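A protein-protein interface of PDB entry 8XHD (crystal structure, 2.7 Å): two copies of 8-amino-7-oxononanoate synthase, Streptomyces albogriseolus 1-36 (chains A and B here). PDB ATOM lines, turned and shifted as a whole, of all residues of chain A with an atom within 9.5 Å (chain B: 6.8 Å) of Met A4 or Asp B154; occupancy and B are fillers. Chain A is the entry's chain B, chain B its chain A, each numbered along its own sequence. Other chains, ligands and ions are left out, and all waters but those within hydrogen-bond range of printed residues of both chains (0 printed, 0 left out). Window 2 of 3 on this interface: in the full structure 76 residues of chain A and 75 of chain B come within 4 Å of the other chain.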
ATOM      1  N   GLY A   1       5.280 -36.328  25.259  1.00  0.00           N
ATOM      2  CA  GLY A   1       6.173 -35.242  25.617  1.00  0.00           C
ATOM      3  C   GLY A   1       5.577 -33.882  25.319  1.00  0.00           C
ATOM      4  O   GLY A   1       4.857 -33.717  24.335  1.00  0.00           O
ATOM      5  N   SER A   2       5.875 -32.902  26.168  1.00  0.00           N
ATOM      6  CA  SER A   2       5.325 -31.562  26.007  1.00  0.00           C
ATOM      7  C   SER A   2       6.232 -30.564  26.717  1.00  0.00           C
ATOM      8  O   SER A   2       7.239 -30.928  27.329  1.00  0.00           O
ATOM      9  CB  SER A   2       3.891 -31.487  26.538  1.00  0.00           C
ATOM     10  OG  SER A   2       3.831 -31.889  27.896  1.00  0.00           O
ATOM     11  N   HIS A   3       5.853 -29.290  26.626  1.00  0.00           N
ATOM     12  CA  HIS A   3       6.595 -28.178  27.205  1.00  0.00           C
ATOM     13  C   HIS A   3       5.637 -27.004  27.365  1.00  0.00           C
ATOM     14  O   HIS A   3       5.732 -26.010  26.638  1.00  0.00           O
ATOM     15  CB  HIS A   3       7.785 -27.813  26.312  1.00  0.00           C
ATOM     16  CG  HIS A   3       8.668 -26.738  26.866  1.00  0.00           C
ATOM     17  ND1 HIS A   3       9.719 -27.002  27.719  1.00  0.00           N
ATOM     18  CD2 HIS A   3       8.674 -25.398  26.669  1.00  0.00           C
ATOM     19  CE1 HIS A   3      10.324 -25.871  28.033  1.00  0.00           C
ATOM     20  NE2 HIS A   3       9.711 -24.882  27.409  1.00  0.00           N
ATOM     21  N   MET A   4       4.707 -27.118  28.307  1.00  0.00           N
ATOM     22  CA  MET A   4       3.533 -26.260  28.328  1.00  0.00           C
ATOM     23  C   MET A   4       3.777 -24.960  29.091  1.00  0.00           C
ATOM     24  O   MET A   4       4.667 -24.853  29.938  1.00  0.00           O
ATOM     25  CB  MET A   4       2.342 -27.002  28.931  1.00  0.00           C
ATOM     26  CG  MET A   4       1.568 -27.828  27.919  1.00  0.00           C
ATOM     27  SD  MET A   4       0.619 -29.133  28.710  1.00  0.00           S
ATOM     28  CE  MET A   4       1.934 -29.975  29.587  1.00  0.00           C
ATOM     29  N   VAL A   5       2.945 -23.966  28.772  1.00  0.00           N
ATOM     30  CA  VAL A   5       3.072 -22.637  29.357  1.00  0.00           C
ATOM     31  C   VAL A   5       2.798 -22.697  30.852  1.00  0.00           C
ATOM     32  O   VAL A   5       1.822 -23.312  31.301  1.00  0.00           O
ATOM     33  CB  VAL A   5       2.115 -21.663  28.653  1.00  0.00           C
ATOM     34  CG1 VAL A   5       2.188 -20.285  29.283  1.00  0.00           C
ATOM     35  CG2 VAL A   5       2.427 -21.587  27.165  1.00  0.00           C
ATOM     36  N   LYS A   6       3.667 -22.058  31.633  1.00  0.00           N
ATOM     37  CA  LYS A   6       3.458 -21.947  33.071  1.00  0.00           C
ATOM     38  C   LYS A   6       2.262 -21.040  33.350  1.00  0.00           C
ATOM     39  O   LYS A   6       2.278 -19.856  32.993  1.00  0.00           O
ATOM     40  CB  LYS A   6       4.718 -21.406  33.743  1.00  0.00           C
ATOM     41  CG  LYS A   6       4.472 -20.749  35.092  1.00  0.00           C
ATOM     42  CD  LYS A   6       5.702 -20.003  35.585  1.00  0.00           C
ATOM     43  CE  LYS A   6       6.747 -20.969  36.096  1.00  0.00           C
ATOM     44  NZ  LYS A   6       6.172 -21.855  37.143  1.00  0.00           N
ATOM     45  N   LYS A   7       1.225 -21.595  33.982  1.00  0.00           N
ATOM     46  CA  LYS A   7      -0.015 -20.857  34.203  1.00  0.00           C
ATOM     47  C   LYS A   7      -0.014 -20.057  35.498  1.00  0.00           C
ATOM     48  O   LYS A   7      -0.709 -19.038  35.590  1.00  0.00           O
ATOM     49  CB  LYS A   7      -1.206 -21.816  34.218  1.00  0.00           C
ATOM     50  CG  LYS A   7      -1.245 -22.791  33.063  1.00  0.00           C
ATOM     51  CD  LYS A   7      -1.731 -22.140  31.788  1.00  0.00           C
ATOM     52  CE  LYS A   7      -2.018 -23.203  30.750  1.00  0.00           C
ATOM     53  NZ  LYS A   7      -0.840 -24.097  30.564  1.00  0.00           N
ATOM     54  N   LEU A   8       0.741 -20.499  36.500  1.00  0.00           N
ATOM     55  CA  LEU A   8       0.765 -19.872  37.817  1.00  0.00           C
ATOM     56  C   LEU A   8       1.984 -18.961  37.894  1.00  0.00           C
ATOM     57  O   LEU A   8       3.122 -19.439  37.906  1.00  0.00           O
ATOM     58  CB  LEU A   8       0.803 -20.939  38.909  1.00  0.00           C
ATOM     59  CG  LEU A   8      -0.215 -22.064  38.721  1.00  0.00           C
ATOM     60  CD1 LEU A   8       0.016 -23.185  39.724  1.00  0.00           C
ATOM     61  CD2 LEU A   8      -1.631 -21.518  38.831  1.00  0.00           C
ATOM     62  N   ARG A   9       1.750 -17.648  37.957  1.00  0.00           N
ATOM     63  CA  ARG A   9       2.846 -16.693  37.863  1.00  0.00           C
ATOM     64  C   ARG A   9       2.864 -15.655  38.979  1.00  0.00           C
ATOM     65  O   ARG A   9       3.578 -14.655  38.855  1.00  0.00           O
ATOM     66  CB  ARG A   9       2.811 -15.984  36.505  1.00  0.00           C
ATOM     67  CG  ARG A   9       2.946 -16.935  35.326  1.00  0.00           C
ATOM     68  CD  ARG A   9       3.136 -16.197  34.014  1.00  0.00           C
ATOM     69  NE  ARG A   9       3.588 -17.097  32.960  1.00  0.00           N
ATOM     70  CZ  ARG A   9       3.835 -16.727  31.712  1.00  0.00           C
ATOM     71  NH1 ARG A   9       3.674 -15.475  31.317  1.00  0.00           N
ATOM     72  NH2 ARG A   9       4.255 -17.636  30.837  1.00  0.00           N
ATOM     73  N   PHE A 143      15.808 -25.068  26.136  1.00  0.00           N
ATOM     74  CA  PHE A 143      14.375 -24.996  25.889  1.00  0.00           C
ATOM     75  C   PHE A 143      14.038 -24.667  24.441  1.00  0.00           C
ATOM     76  O   PHE A 143      12.882 -24.836  24.036  1.00  0.00           O
ATOM     77  CB  PHE A 143      13.736 -23.977  26.837  1.00  0.00           C
ATOM     78  CG  PHE A 143      13.477 -24.521  28.216  1.00  0.00           C
ATOM     79  CD1 PHE A 143      13.847 -25.816  28.544  1.00  0.00           C
ATOM     80  CD2 PHE A 143      12.844 -23.749  29.177  1.00  0.00           C
ATOM     81  CE1 PHE A 143      13.603 -26.326  29.807  1.00  0.00           C
ATOM     82  CE2 PHE A 143      12.594 -24.255  30.441  1.00  0.00           C
ATOM     83  CZ  PHE A 143      12.975 -25.544  30.755  1.00  0.00           C
ATOM     84  N   ALA A 146      13.541 -28.246  23.681  1.00  0.00           N
ATOM     85  CA  ALA A 146      12.549 -28.956  24.480  1.00  0.00           C
ATOM     86  C   ALA A 146      11.133 -28.456  24.213  1.00  0.00           C
ATOM     87  O   ALA A 146      10.169 -29.211  24.383  1.00  0.00           O
ATOM     88  CB  ALA A 146      12.888 -28.831  25.965  1.00  0.00           C
ATOM     89  N   SER A 147      10.983 -27.200  23.790  1.00  0.00           N
ATOM     90  CA  SER A 147       9.655 -26.670  23.496  1.00  0.00           C
ATOM     91  C   SER A 147       9.025 -27.324  22.272  1.00  0.00           C
ATOM     92  O   SER A 147       7.808 -27.215  22.080  1.00  0.00           O
ATOM     93  CB  SER A 147       9.727 -25.156  23.297  1.00  0.00           C
ATOM     94  OG  SER A 147      10.736 -24.816  22.365  1.00  0.00           O
ATOM     95  N   LEU A 148       9.818 -28.010  21.451  1.00  0.00           N
ATOM     96  CA  LEU A 148       9.338 -28.625  20.224  1.00  0.00           C
ATOM     97  C   LEU A 148       9.103 -30.126  20.376  1.00  0.00           C
ATOM     98  O   LEU A 148       9.017 -30.837  19.370  1.00  0.00           O
ATOM     99  CB  LEU A 148      10.327 -28.350  19.090  1.00  0.00           C
ATOM    100  CG  LEU A 148      10.697 -26.874  18.915  1.00  0.00           C
ATOM    101  CD1 LEU A 148      11.873 -26.731  17.973  1.00  0.00           C
ATOM    102  CD2 LEU A 148       9.509 -26.071  18.410  1.00  0.00           C
ATOM    103  N   LYS A 149       9.005 -30.620  21.615  1.00  0.00           N
ATOM    104  CA  LYS A 149       8.722 -32.037  21.831  1.00  0.00           C
ATOM    105  C   LYS A 149       7.362 -32.414  21.260  1.00  0.00           C
ATOM    106  O   LYS A 149       7.200 -33.500  20.693  1.00  0.00           O
ATOM    107  CB  LYS A 149       8.779 -32.367  23.324  1.00  0.00           C
ATOM    108  CG  LYS A 149      10.164 -32.302  23.940  1.00  0.00           C
ATOM    109  CD  LYS A 149      10.111 -32.601  25.431  1.00  0.00           C
ATOM    110  CE  LYS A 149      11.480 -32.460  26.071  1.00  0.00           C
ATOM    111  NZ  LYS A 149      11.450 -32.754  27.531  1.00  0.00           N
ATOM    112  N   SER A 150       6.373 -31.529  21.410  1.00  0.00           N
ATOM    113  CA  SER A 150       5.037 -31.804  20.893  1.00  0.00           C
ATOM    114  C   SER A 150       5.050 -31.951  19.380  1.00  0.00           C
ATOM    115  O   SER A 150       4.315 -32.776  18.825  1.00  0.00           O
ATOM    116  CB  SER A 150       4.080 -30.693  21.312  1.00  0.00           C
ATOM    117  OG  SER A 150       4.380 -30.239  22.620  1.00  0.00           O
ATOM    118  N   LEU A 151       5.870 -31.149  18.693  1.00  0.00           N
ATOM    119  CA  LEU A 151       6.041 -31.327  17.257  1.00  0.00           C
ATOM    120  C   LEU A 151       6.636 -32.692  16.954  1.00  0.00           C
ATOM    121  O   LEU A 151       6.211 -33.372  16.013  1.00  0.00           O
ATOM    122  CB  LEU A 151       6.929 -30.220  16.691  1.00  0.00           C
ATOM    123  CG  LEU A 151       6.236 -29.028  16.034  1.00  0.00           C
ATOM    124  CD1 LEU A 151       5.132 -28.484  16.925  1.00  0.00           C
ATOM    125  CD2 LEU A 151       7.248 -27.939  15.709  1.00  0.00           C
ATOM    126  N   CYS A 152       7.622 -33.109  17.747  1.00  0.00           N
ATOM    127  CA  CYS A 152       8.239 -34.413  17.544  1.00  0.00           C
ATOM    128  C   CYS A 152       7.280 -35.544  17.890  1.00  0.00           C
ATOM    129  O   CYS A 152       7.327 -36.607  17.262  1.00  0.00           O
ATOM    130  CB  CYS A 152       9.515 -34.515  18.378  1.00  0.00           C
ATOM    131  SG  CYS A 152      10.763 -33.274  17.965  1.00  0.00           S
ATOM    132  N   ALA A 153       6.401 -35.330  18.874  1.00  0.00           N
ATOM    133  CA  ALA A 153       5.443 -36.355  19.272  1.00  0.00           C
ATOM    134  C   ALA A 153       4.409 -36.639  18.191  1.00  0.00           C
ATOM    135  O   ALA A 153       3.761 -37.690  18.232  1.00  0.00           O
ATOM    136  CB  ALA A 153       4.738 -35.945  20.566  1.00  0.00           C
ATOM    137  N   ASP A 154       4.231 -35.722  17.237  1.00  0.00           N
ATOM    138  CA  ASP A 154       3.353 -35.984  16.103  1.00  0.00           C
ATOM    139  C   ASP A 154       3.940 -37.006  15.140  1.00  0.00           C
ATOM    140  O   ASP A 154       3.199 -37.572  14.330  1.00  0.00           O
ATOM    141  CB  ASP A 154       3.067 -34.686  15.345  1.00  0.00           C
ATOM    142  CG  ASP A 154       2.210 -33.723  16.136  1.00  0.00           C
ATOM    143  OD1 ASP A 154       1.721 -34.105  17.220  1.00  0.00           O
ATOM    144  OD2 ASP A 154       2.026 -32.580  15.669  1.00  0.00           O
ATOM    145  N   LYS B 149       0.498 -25.865  15.559  1.00  0.00           N
ATOM    146  CA  LYS B 149      -0.822 -26.237  16.059  1.00  0.00           C
ATOM    147  C   LYS B 149      -0.708 -27.203  17.229  1.00  0.00           C
ATOM    148  O   LYS B 149      -1.487 -27.127  18.186  1.00  0.00           O
ATOM    149  CB  LYS B 149      -1.657 -26.861  14.940  1.00  0.00           C
ATOM    150  CG  LYS B 149      -2.148 -25.889  13.886  1.00  0.00           C
ATOM    151  CD  LYS B 149      -2.900 -26.630  12.789  1.00  0.00           C
ATOM    152  CE  LYS B 149      -3.289 -25.698  11.653  1.00  0.00           C
ATOM    153  NZ  LYS B 149      -3.886 -26.433  10.503  1.00  0.00           N
ATOM    154  N   SER B 150       0.256 -28.125  17.163  1.00  0.00           N
ATOM    155  CA  SER B 150       0.422 -29.109  18.226  1.00  0.00           C
ATOM    156  C   SER B 150       0.815 -28.444  19.539  1.00  0.00           C
ATOM    157  O   SER B 150       0.371 -28.869  20.612  1.00  0.00           O
ATOM    158  CB  SER B 150       1.463 -30.145  17.818  1.00  0.00           C
ATOM    159  OG  SER B 150       1.125 -30.729  16.573  1.00  0.00           O
ATOM    160  N   LEU B 151       1.654 -27.408  19.474  1.00  0.00           N
ATOM    161  CA  LEU B 151       1.982 -26.640  20.669  1.00  0.00           C
ATOM    162  C   LEU B 151       0.733 -25.991  21.245  1.00  0.00           C
ATOM    163  O   LEU B 151       0.518 -25.995  22.463  1.00  0.00           O
ATOM    164  CB  LEU B 151       3.035 -25.581  20.339  1.00  0.00           C
ATOM    165  CG  LEU B 151       4.489 -25.898  20.689  1.00  0.00           C
ATOM    166  CD1 LEU B 151       4.839 -27.319  20.296  1.00  0.00           C
ATOM    167  CD2 LEU B 151       5.426 -24.909  20.011  1.00  0.00           C
ATOM    168  N   CYS B 152      -0.102 -25.417  20.374  1.00  0.00           N
ATOM    169  CA  CYS B 152      -1.363 -24.841  20.825  1.00  0.00           C
ATOM    170  C   CYS B 152      -2.329 -25.915  21.299  1.00  0.00           C
ATOM    171  O   CYS B 152      -3.119 -25.680  22.222  1.00  0.00           O
ATOM    172  CB  CYS B 152      -1.994 -24.025  19.700  1.00  0.00           C
ATOM    173  SG  CYS B 152      -0.985 -22.650  19.116  1.00  0.00           S
ATOM    174  N   ALA B 153      -2.274 -27.103  20.687  1.00  0.00           N
ATOM    175  CA  ALA B 153      -3.203 -28.173  21.035  1.00  0.00           C
ATOM    176  C   ALA B 153      -2.954 -28.707  22.438  1.00  0.00           C
ATOM    177  O   ALA B 153      -3.900 -29.125  23.114  1.00  0.00           O
ATOM    178  CB  ALA B 153      -3.102 -29.309  20.015  1.00  0.00           C
ATOM    179  N   ASP B 154      -1.697 -28.715  22.884  1.00  0.00           N
ATOM    180  CA  ASP B 154      -1.394 -29.132  24.247  1.00  0.00           C
ATOM    181  C   ASP B 154      -1.980 -28.176  25.274  1.00  0.00           C
ATOM    182  O   ASP B 154      -2.067 -28.525  26.456  1.00  0.00           O
ATOM    183  CB  ASP B 154       0.119 -29.240  24.448  1.00  0.00           C
ATOM    184  CG  ASP B 154       0.732 -30.397  23.683  1.00  0.00           C
ATOM    185  OD1 ASP B 154      -0.017 -31.126  23.001  1.00  0.00           O
ATOM    186  OD2 ASP B 154       1.965 -30.577  23.770  1.00  0.00           O
ATOM    187  N   GLU B 155      -2.385 -26.980  24.849  1.00  0.00           N
ATOM    188  CA  GLU B 155      -2.907 -25.973  25.757  1.00  0.00           C
ATOM    189  C   GLU B 155      -4.421 -25.835  25.692  1.00  0.00           C
ATOM    190  O   GLU B 155      -5.028 -25.421  26.686  1.00  0.00           O
ATOM    191  CB  GLU B 155      -2.263 -24.611  25.458  1.00  0.00           C
ATOM    192  CG  GLU B 155      -0.745 -24.584  25.575  1.00  0.00           C
ATOM    193  CD  GLU B 155      -0.265 -24.510  27.013  1.00  0.00           C
ATOM    194  OE1 GLU B 155      -1.108 -24.320  27.913  1.00  0.00           O
ATOM    195  OE2 GLU B 155       0.955 -24.641  27.243  1.00  0.00           O
ATOM    196  N   THR B 156      -5.042 -26.169  24.565  1.00  0.00           N
ATOM    197  CA  THR B 156      -6.470 -25.934  24.360  1.00  0.00           C
ATOM    198  C   THR B 156      -6.919 -26.714  23.128  1.00  0.00           C
ATOM    199  O   THR B 156      -6.178 -27.550  22.596  1.00  0.00           O
ATOM    200  CB  THR B 156      -6.766 -24.444  24.204  1.00  0.00           C
ATOM    201  OG1 THR B 156      -8.177 -24.246  24.080  1.00  0.00           O
ATOM    202  CG2 THR B 156      -6.070 -23.895  22.966  1.00  0.00           C
ATOM    203  N   VAL B 158      -7.793 -27.014  19.238  1.00  0.00           N
ATOM    204  CA  VAL B 158      -7.365 -26.422  17.975  1.00  0.00           C
ATOM    205  C   VAL B 158      -8.289 -26.912  16.869  1.00  0.00           C
ATOM    206  O   VAL B 158      -8.482 -28.121  16.700  1.00  0.00           O
ATOM    207  CB  VAL B 158      -5.900 -26.765  17.652  1.00  0.00           C
ATOM    208  CG1 VAL B 158      -5.545 -26.304  16.244  1.00  0.00           C
ATOM    209  CG2 VAL B 158      -4.973 -26.124  18.668  1.00  0.00           C
ATOM    210  N   SER B 275       8.402 -19.014  28.253  1.00  0.00           N
ATOM    211  CA  SER B 275       9.525 -19.760  27.692  1.00  0.00           C
ATOM    212  C   SER B 275       9.360 -19.797  26.178  1.00  0.00           C
ATOM    213  O   SER B 275       8.701 -20.678  25.622  1.00  0.00           O
ATOM    214  CB  SER B 275       9.588 -21.157  28.292  1.00  0.00           C
ATOM    215  OG  SER B 275      10.837 -21.768  28.023  1.00  0.00           O
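The side-chain carboxylate (OD2) of Asp B154 sits at hydrogen-bond distance from the side-chain hydroxyl (OG) of Ser A150, 2.7 Å away. OE1 of Glu B155 lies within salt-bridge range of NZ of Lys A7 (2.7 Å). The backbone carbonyl oxygen (O) of Asp B154 sits close to the side-chain sulfur (SD) of Met A4. The side-chain hydroxyl of Ser B275 sits at hydrogen-bond distance from a ring nitrogen (NE2) of His A3. The side-chain carboxylate of Asp A154 sits close to the side-chain hydroxyl of Ser B150 (3.5 Å). The backbone NH (N) of Val A5 lies within hydrogen-bond range of the side-chain carboxylate (OE2) of Glu B155 (2.6 Å).
O of Val A5 is in hydrogen-bond range of NZ of Lys A7 (2.9 Å). OG of Ser A147 lies within hydrogen-bond range of O of Phe A143.
Asp B154 touches Ser A2 (OD2 to CB, 3.5 Å). OE2 of Glu B155 touches CB of Met A4, at 3.2 Å. OG of Ser B275 touches CD2 of Phe A143, at 3.0 Å. Leu B151 touches Ser A147 (CD1 to O, 3.5 Å). CD1 of Leu B151 touches CB of Ser A150, 3.6 Å away. Leu A151 touches Leu B151.
Of chain B, only Asp B154 (3.6 Å) and Glu B155 (3.2 Å) come within 4 Å of Met A4. Lys A6 touches none of the printed residues of chain B. Printed residues of chain B within 4 Å of Phe A143: Ser B275 (3.0 Å). Of the printed residues of chain B, Ser A150 touches Leu B151 (3.6 Å) and Asp B154 (2.7 Å). Printed residues of chain A within 4 Å of Ser B150: Asp A154. Cys B152 touches none of the printed residues of chain A. No residue of chain A comes within 4 Å of Ala B153. Of the printed residues of chain A, Asp B154 touches Ser A2, Met A4 and Ser A150.
Of the 19 printed residues of chain A, 10 touch a printed residue of chain B. Printed residues of chain A that touch a printed residue of chain B: Ser A2, His A3, Met A4, Val A5, Lys A7, Phe A143, Ser A147, Ser A150, Leu A151 and Asp A154. Of the 10 printed residues of chain B, 5 touch a printed residue of chain A. Hydrophobic or aromatic side chains of chain B that line the printed part of chain A: Leu B151. Among the printed residues, Asp or Glu carboxylates within 4 Å of a Lys or Arg side-chain nitrogen of the other chain: Lys A7 with Glu B155 (2.7 Å).
Ser A150 touches Leu B151, but with the chains exchanged Leu A151 does not touch Ser B150 (4.1 Å). Ser A150 touches Asp B154, and with the chains exchanged Asp A154 touches Ser B150. Leu B151 touches its own counterpart, Leu A151. Of the 12 pairs that touch across the chains among the printed residues, 3 have their exchanged pair printed and touching as well.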
